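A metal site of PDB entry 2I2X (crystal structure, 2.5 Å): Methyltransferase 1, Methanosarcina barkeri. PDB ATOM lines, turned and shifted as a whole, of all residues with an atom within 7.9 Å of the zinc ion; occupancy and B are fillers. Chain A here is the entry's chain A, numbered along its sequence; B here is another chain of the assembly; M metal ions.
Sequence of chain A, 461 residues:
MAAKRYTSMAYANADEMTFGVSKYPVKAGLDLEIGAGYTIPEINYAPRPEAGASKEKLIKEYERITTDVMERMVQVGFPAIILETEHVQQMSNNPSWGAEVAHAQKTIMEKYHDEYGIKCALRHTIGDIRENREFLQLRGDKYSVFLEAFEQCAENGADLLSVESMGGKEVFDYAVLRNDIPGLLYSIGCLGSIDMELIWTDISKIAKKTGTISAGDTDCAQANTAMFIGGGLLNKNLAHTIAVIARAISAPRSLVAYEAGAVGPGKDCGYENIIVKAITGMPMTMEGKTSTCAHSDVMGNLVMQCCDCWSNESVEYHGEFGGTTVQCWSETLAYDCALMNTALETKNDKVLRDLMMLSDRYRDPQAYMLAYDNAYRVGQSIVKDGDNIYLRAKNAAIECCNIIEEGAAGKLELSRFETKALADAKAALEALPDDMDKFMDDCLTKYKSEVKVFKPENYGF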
ATOM      1  N   CYS A 293       7.376  -7.024  17.303  1.00  0.00           N
ATOM      2  CA  CYS A 293       6.616  -6.065  16.480  1.00  0.00           C
ATOM      3  C   CYS A 293       5.338  -6.680  15.893  1.00  0.00           C
ATOM      4  O   CYS A 293       4.328  -5.995  15.664  1.00  0.00           O
ATOM      5  CB  CYS A 293       7.480  -5.534  15.341  1.00  0.00           C
ATOM      6  SG  CYS A 293       8.578  -6.795  14.588  1.00  0.00           S
ATOM      7  N   VAL A 315       6.076  -6.207  10.439  1.00  0.00           N
ATOM      8  CA  VAL A 315       5.886  -4.908  11.034  1.00  0.00           C
ATOM      9  C   VAL A 315       5.386  -3.979   9.924  1.00  0.00           C
ATOM     10  O   VAL A 315       5.781  -4.147   8.750  1.00  0.00           O
ATOM     11  CB  VAL A 315       7.226  -4.373  11.602  1.00  0.00           C
ATOM     12  CG1 VAL A 315       8.275  -4.135  10.471  1.00  0.00           C
ATOM     13  CG2 VAL A 315       7.014  -3.110  12.499  1.00  0.00           C
ATOM     14  N   GLU A 316       4.540  -3.018  10.273  1.00  0.00           N
ATOM     15  CA  GLU A 316       4.123  -2.001   9.319  1.00  0.00           C
ATOM     16  C   GLU A 316       5.294  -1.106   8.938  1.00  0.00           C
ATOM     17  O   GLU A 316       6.075  -0.723   9.783  1.00  0.00           O
ATOM     18  CB  GLU A 316       3.006  -1.117   9.858  1.00  0.00           C
ATOM     19  CG  GLU A 316       2.536  -0.124   8.810  1.00  0.00           C
ATOM     20  CD  GLU A 316       1.504   0.804   9.327  1.00  0.00           C
ATOM     21  OE1 GLU A 316       0.342   0.664   8.882  1.00  0.00           O
ATOM     22  OE2 GLU A 316       1.859   1.663  10.201  1.00  0.00           O
ATOM     23  N   TYR A 317       5.407  -0.782   7.665  1.00  0.00           N
ATOM     24  CA  TYR A 317       6.413   0.157   7.243  1.00  0.00           C
ATOM     25  C   TYR A 317       6.036   1.585   7.683  1.00  0.00           C
ATOM     26  O   TYR A 317       5.108   2.183   7.113  1.00  0.00           O
ATOM     27  CB  TYR A 317       6.609   0.086   5.729  1.00  0.00           C
ATOM     28  CG  TYR A 317       7.667   1.012   5.210  1.00  0.00           C
ATOM     29  CD1 TYR A 317       8.994   0.890   5.644  1.00  0.00           C
ATOM     30  CD2 TYR A 317       7.354   1.998   4.274  1.00  0.00           C
ATOM     31  CE1 TYR A 317      10.000   1.742   5.170  1.00  0.00           C
ATOM     32  CE2 TYR A 317       8.372   2.863   3.762  1.00  0.00           C
ATOM     33  CZ  TYR A 317       9.685   2.720   4.222  1.00  0.00           C
ATOM     34  OH  TYR A 317      10.668   3.562   3.751  1.00  0.00           O
ATOM     35  N   HIS A 318       6.723   2.109   8.695  1.00  0.00           N
ATOM     36  CA  HIS A 318       6.521   3.505   9.104  1.00  0.00           C
ATOM     37  C   HIS A 318       7.742   4.071   9.841  1.00  0.00           C
ATOM     38  O   HIS A 318       8.716   3.347  10.079  1.00  0.00           O
ATOM     39  CB  HIS A 318       5.197   3.703   9.884  1.00  0.00           C
ATOM     40  CG  HIS A 318       5.150   3.042  11.238  1.00  0.00           C
ATOM     41  ND1 HIS A 318       4.197   2.089  11.562  1.00  0.00           N
ATOM     42  CD2 HIS A 318       5.898   3.215  12.351  1.00  0.00           C
ATOM     43  CE1 HIS A 318       4.372   1.709  12.813  1.00  0.00           C
ATOM     44  NE2 HIS A 318       5.405   2.364  13.310  1.00  0.00           N
ATOM     45  N   GLY A 319       7.690   5.358  10.189  1.00  0.00           N
ATOM     46  CA  GLY A 319       8.810   6.060  10.845  1.00  0.00           C
ATOM     47  C   GLY A 319       8.935   5.758  12.332  1.00  0.00           C
ATOM     48  O   GLY A 319       7.907   5.670  13.022  1.00  0.00           O
ATOM     49  N   GLU A 320      10.160   5.558  12.825  1.00  0.00           N
ATOM     50  CA  GLU A 320      10.464   5.465  14.269  1.00  0.00           C
ATOM     51  C   GLU A 320      11.584   6.482  14.548  1.00  0.00           C
ATOM     52  O   GLU A 320      12.193   6.967  13.583  1.00  0.00           O
ATOM     53  CB  GLU A 320      11.019   4.069  14.618  1.00  0.00           C
ATOM     54  CG  GLU A 320      10.087   2.857  14.452  1.00  0.00           C
ATOM     55  CD  GLU A 320       8.798   2.947  15.257  1.00  0.00           C
ATOM     56  OE1 GLU A 320       8.750   3.705  16.252  1.00  0.00           O
ATOM     57  OE2 GLU A 320       7.820   2.274  14.865  1.00  0.00           O
ATOM     58  N   PHE A 321      11.920   6.796  15.807  1.00  0.00           N
ATOM     59  CA  PHE A 321      13.017   7.743  16.026  1.00  0.00           C
ATOM     60  C   PHE A 321      14.318   7.317  15.304  1.00  0.00           C
ATOM     61  O   PHE A 321      15.097   8.183  14.885  1.00  0.00           O
ATOM     62  CB  PHE A 321      13.333   7.974  17.512  1.00  0.00           C
ATOM     63  CG  PHE A 321      12.187   8.542  18.321  1.00  0.00           C
ATOM     64  CD1 PHE A 321      11.257   9.447  17.756  1.00  0.00           C
ATOM     65  CD2 PHE A 321      12.056   8.199  19.672  1.00  0.00           C
ATOM     66  CE1 PHE A 321      10.201   9.988  18.555  1.00  0.00           C
ATOM     67  CE2 PHE A 321      10.990   8.711  20.468  1.00  0.00           C
ATOM     68  CZ  PHE A 321      10.067   9.609  19.906  1.00  0.00           C
ATOM     69  N   GLY A 323      14.844   5.597  12.621  1.00  0.00           N
ATOM     70  CA  GLY A 323      14.773   5.353  11.214  1.00  0.00           C
ATOM     71  C   GLY A 323      13.524   4.576  10.874  1.00  0.00           C
ATOM     72  O   GLY A 323      12.514   4.563  11.612  1.00  0.00           O
ATOM     73  N   THR A 325      11.030   1.595  10.277  1.00  0.00           N
ATOM     74  CA  THR A 325      10.723   0.373  10.957  1.00  0.00           C
ATOM     75  C   THR A 325      11.477  -0.875  10.461  1.00  0.00           C
ATOM     76  O   THR A 325      11.958  -1.701  11.276  1.00  0.00           O
ATOM     77  CB  THR A 325       9.229   0.216  10.850  1.00  0.00           C
ATOM     78  OG1 THR A 325       8.769  -0.605  11.895  1.00  0.00           O
ATOM     79  CG2 THR A 325       8.826  -0.309   9.516  1.00  0.00           C
ATOM     80  N   TRP A 329      14.313  -3.019  12.878  1.00  0.00           N
ATOM     81  CA  TRP A 329      14.192  -4.444  13.118  1.00  0.00           C
ATOM     82  C   TRP A 329      15.232  -5.249  12.348  1.00  0.00           C
ATOM     83  O   TRP A 329      15.713  -6.245  12.888  1.00  0.00           O
ATOM     84  CB  TRP A 329      12.779  -4.954  12.906  1.00  0.00           C
ATOM     85  CG  TRP A 329      11.823  -4.455  13.924  1.00  0.00           C
ATOM     86  CD1 TRP A 329      10.983  -3.354  13.815  1.00  0.00           C
ATOM     87  CD2 TRP A 329      11.602  -4.987  15.234  1.00  0.00           C
ATOM     88  NE1 TRP A 329      10.263  -3.193  14.966  1.00  0.00           N
ATOM     89  CE2 TRP A 329      10.623  -4.176  15.856  1.00  0.00           C
ATOM     90  CE3 TRP A 329      12.153  -6.053  15.939  1.00  0.00           C
ATOM     91  CZ2 TRP A 329      10.172  -4.407  17.153  1.00  0.00           C
ATOM     92  CZ3 TRP A 329      11.701  -6.297  17.246  1.00  0.00           C
ATOM     93  CH2 TRP A 329      10.722  -5.466  17.836  1.00  0.00           C
ATOM     94  N   CYS B 293      15.172   1.160  17.718  1.00  0.00           N
ATOM     95  CA  CYS B 293      14.025   2.042  17.713  1.00  0.00           C
ATOM     96  C   CYS B 293      14.468   3.537  17.898  1.00  0.00           C
ATOM     97  O   CYS B 293      13.789   4.464  17.404  1.00  0.00           O
ATOM     98  CB  CYS B 293      13.008   1.604  18.784  1.00  0.00           C
ATOM     99  SG  CYS B 293      13.679   1.323  20.492  1.00  0.00           S
ATOM    100  N   VAL B 315      11.543   5.198  22.302  1.00  0.00           N
ATOM    101  CA  VAL B 315      10.666   4.882  21.176  1.00  0.00           C
ATOM    102  C   VAL B 315       9.383   5.677  21.410  1.00  0.00           C
ATOM    103  O   VAL B 315       8.911   5.779  22.567  1.00  0.00           O
ATOM    104  CB  VAL B 315      10.352   3.372  21.123  1.00  0.00           C
ATOM    105  CG1 VAL B 315       9.502   2.925  22.341  1.00  0.00           C
ATOM    106  CG2 VAL B 315       9.669   2.953  19.792  1.00  0.00           C
ATOM    107  N   GLU B 316       8.785   6.264  20.375  1.00  0.00           N
ATOM    108  CA  GLU B 316       7.475   6.899  20.611  1.00  0.00           C
ATOM    109  C   GLU B 316       6.464   5.848  21.086  1.00  0.00           C
ATOM    110  O   GLU B 316       6.518   4.713  20.641  1.00  0.00           O
ATOM    111  CB  GLU B 316       6.962   7.642  19.371  1.00  0.00           C
ATOM    112  CG  GLU B 316       5.603   8.334  19.578  1.00  0.00           C
ATOM    113  CD  GLU B 316       5.002   8.901  18.287  1.00  0.00           C
ATOM    114  OE1 GLU B 316       4.972  10.138  18.174  1.00  0.00           O
ATOM    115  OE2 GLU B 316       4.569   8.119  17.393  1.00  0.00           O
ATOM    116  N   TYR B 317       5.542   6.230  21.968  1.00  0.00           N
ATOM    117  CA  TYR B 317       4.457   5.366  22.371  1.00  0.00           C
ATOM    118  C   TYR B 317       3.391   5.347  21.289  1.00  0.00           C
ATOM    119  O   TYR B 317       2.711   6.361  21.102  1.00  0.00           O
ATOM    120  CB  TYR B 317       3.806   5.918  23.637  1.00  0.00           C
ATOM    121  CG  TYR B 317       2.702   5.045  24.182  1.00  0.00           C
ATOM    122  CD1 TYR B 317       2.970   3.753  24.659  1.00  0.00           C
ATOM    123  CD2 TYR B 317       1.382   5.476  24.205  1.00  0.00           C
ATOM    124  CE1 TYR B 317       1.971   2.931  25.145  1.00  0.00           C
ATOM    125  CE2 TYR B 317       0.354   4.645  24.712  1.00  0.00           C
ATOM    126  CZ  TYR B 317       0.676   3.379  25.177  1.00  0.00           C
ATOM    127  OH  TYR B 317      -0.292   2.555  25.685  1.00  0.00           O
ATOM    128  N   HIS B 318       3.245   4.226  20.579  1.00  0.00           N
ATOM    129  CA  HIS B 318       2.170   4.061  19.591  1.00  0.00           C
ATOM    130  C   HIS B 318       1.940   2.566  19.239  1.00  0.00           C
ATOM    131  O   HIS B 318       2.664   1.691  19.696  1.00  0.00           O
ATOM    132  CB  HIS B 318       2.419   4.891  18.330  1.00  0.00           C
ATOM    133  CG  HIS B 318       3.595   4.454  17.520  1.00  0.00           C
ATOM    134  ND1 HIS B 318       4.686   5.270  17.280  1.00  0.00           N
ATOM    135  CD2 HIS B 318       3.844   3.293  16.859  1.00  0.00           C
ATOM    136  CE1 HIS B 318       5.559   4.626  16.521  1.00  0.00           C
ATOM    137  NE2 HIS B 318       5.083   3.416  16.267  1.00  0.00           N
ATOM    138  N   GLY B 319       0.923   2.287  18.423  1.00  0.00           N
ATOM    139  CA  GLY B 319       0.566   0.880  18.098  1.00  0.00           C
ATOM    140  C   GLY B 319       1.465   0.196  17.072  1.00  0.00           C
ATOM    141  O   GLY B 319       1.994   0.831  16.150  1.00  0.00           O
ATOM    142  N   GLU B 320       1.676  -1.110  17.273  1.00  0.00           N
ATOM    143  CA  GLU B 320       2.311  -1.990  16.291  1.00  0.00           C
ATOM    144  C   GLU B 320       1.383  -3.184  16.191  1.00  0.00           C
ATOM    145  O   GLU B 320       0.472  -3.316  17.010  1.00  0.00           O
ATOM    146  CB  GLU B 320       3.689  -2.437  16.801  1.00  0.00           C
ATOM    147  CG  GLU B 320       4.653  -1.290  17.171  1.00  0.00           C
ATOM    148  CD  GLU B 320       5.242  -0.571  15.950  1.00  0.00           C
ATOM    149  OE1 GLU B 320       5.185  -1.119  14.840  1.00  0.00           O
ATOM    150  OE2 GLU B 320       5.766   0.539  16.107  1.00  0.00           O
ATOM    151  N   PHE B 321       1.607  -4.085  15.241  1.00  0.00           N
ATOM    152  CA  PHE B 321       0.763  -5.288  15.182  1.00  0.00           C
ATOM    153  C   PHE B 321       0.833  -6.095  16.517  1.00  0.00           C
ATOM    154  O   PHE B 321      -0.151  -6.741  16.921  1.00  0.00           O
ATOM    155  CB  PHE B 321       1.130  -6.222  13.997  1.00  0.00           C
ATOM    156  CG  PHE B 321       1.233  -5.554  12.652  1.00  0.00           C
ATOM    157  CD1 PHE B 321       0.324  -4.582  12.254  1.00  0.00           C
ATOM    158  CD2 PHE B 321       2.209  -5.937  11.768  1.00  0.00           C
ATOM    159  CE1 PHE B 321       0.414  -3.990  10.991  1.00  0.00           C
ATOM    160  CE2 PHE B 321       2.298  -5.367  10.494  1.00  0.00           C
ATOM    161  CZ  PHE B 321       1.398  -4.379  10.110  1.00  0.00           C
ATOM    162  N   GLY B 323       1.235  -5.175  19.570  1.00  0.00           N
ATOM    163  CA  GLY B 323       0.788  -4.457  20.739  1.00  0.00           C
ATOM    164  C   GLY B 323       1.447  -3.097  20.771  1.00  0.00           C
ATOM    165  O   GLY B 323       1.945  -2.547  19.775  1.00  0.00           O
ATOM    166  N   THR B 325       4.065  -0.246  21.362  1.00  0.00           N
ATOM    167  CA  THR B 325       5.484  -0.025  21.196  1.00  0.00           C
ATOM    168  C   THR B 325       6.340  -0.375  22.440  1.00  0.00           C
ATOM    169  O   THR B 325       7.420  -1.000  22.332  1.00  0.00           O
ATOM    170  CB  THR B 325       5.640   1.430  20.788  1.00  0.00           C
ATOM    171  OG1 THR B 325       6.576   1.525  19.745  1.00  0.00           O
ATOM    172  CG2 THR B 325       6.014   2.275  21.904  1.00  0.00           C
ATOM    173  N   TRP B 329       9.146  -3.649  22.624  1.00  0.00           N
ATOM    174  CA  TRP B 329      10.575  -3.527  23.007  1.00  0.00           C
ATOM    175  C   TRP B 329      10.896  -4.032  24.420  1.00  0.00           C
ATOM    176  O   TRP B 329      12.012  -4.543  24.653  1.00  0.00           O
ATOM    177  CB  TRP B 329      11.112  -2.108  22.770  1.00  0.00           C
ATOM    178  CG  TRP B 329      11.081  -1.715  21.348  1.00  0.00           C
ATOM    179  CD1 TRP B 329      10.072  -1.079  20.716  1.00  0.00           C
ATOM    180  CD2 TRP B 329      12.071  -1.975  20.340  1.00  0.00           C
ATOM    181  NE1 TRP B 329      10.365  -0.902  19.393  1.00  0.00           N
ATOM    182  CE2 TRP B 329      11.595  -1.447  19.137  1.00  0.00           C
ATOM    183  CE3 TRP B 329      13.312  -2.611  20.355  1.00  0.00           C
ATOM    184  CZ2 TRP B 329      12.291  -1.541  17.944  1.00  0.00           C
ATOM    185  CZ3 TRP B 329      14.028  -2.702  19.191  1.00  0.00           C
ATOM    186  CH2 TRP B 329      13.527  -2.169  17.989  1.00  0.00           C
HETATM  187 ZN    ZN M   1       6.086   2.041  15.150  1.00  0.00          ZN
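The backbone NH (N) of Thr 325 of chain A sits at hydrogen-bond distance from the backbone carbonyl oxygen (O) of His 318 of chain A, 2.9 Å away. A ring nitrogen (ND1) of His 318 of chain A lies within hydrogen-bond range of the side-chain carboxylate of Glu 316 of chain A (2.7 Å). The backbone NH (N) of Thr 325 of chain B is in hydrogen-bond range of the backbone carbonyl oxygen (O) of His 318 of chain B. The side-chain carboxylate of Glu 316 of chain B lies within hydrogen-bond range of a ring nitrogen (ND1) of His 318 of chain B, 2.9 Å away.
Of the 22 residues printed, 4 come within 4 Å of the zinc ion. Along chain A the residues within 4 Å of the zinc ion span positions 318 to 320. The nearest printed residue that does not touch the zinc ion is Gly 319 of chain B (4.4 Å).
The zinc ion is bound by the side-chain carboxylate of Glu 320 of chain A (1.8 Å), the side-chain carboxylate of Glu 320 of chain B (1.8 Å), a ring nitrogen (NE2) of His 318 of chain A (2.0 Å) and a ring nitrogen (NE2) of His 318 of chain B (2.0 Å). The zinc ion has four donor atoms within binding distance.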
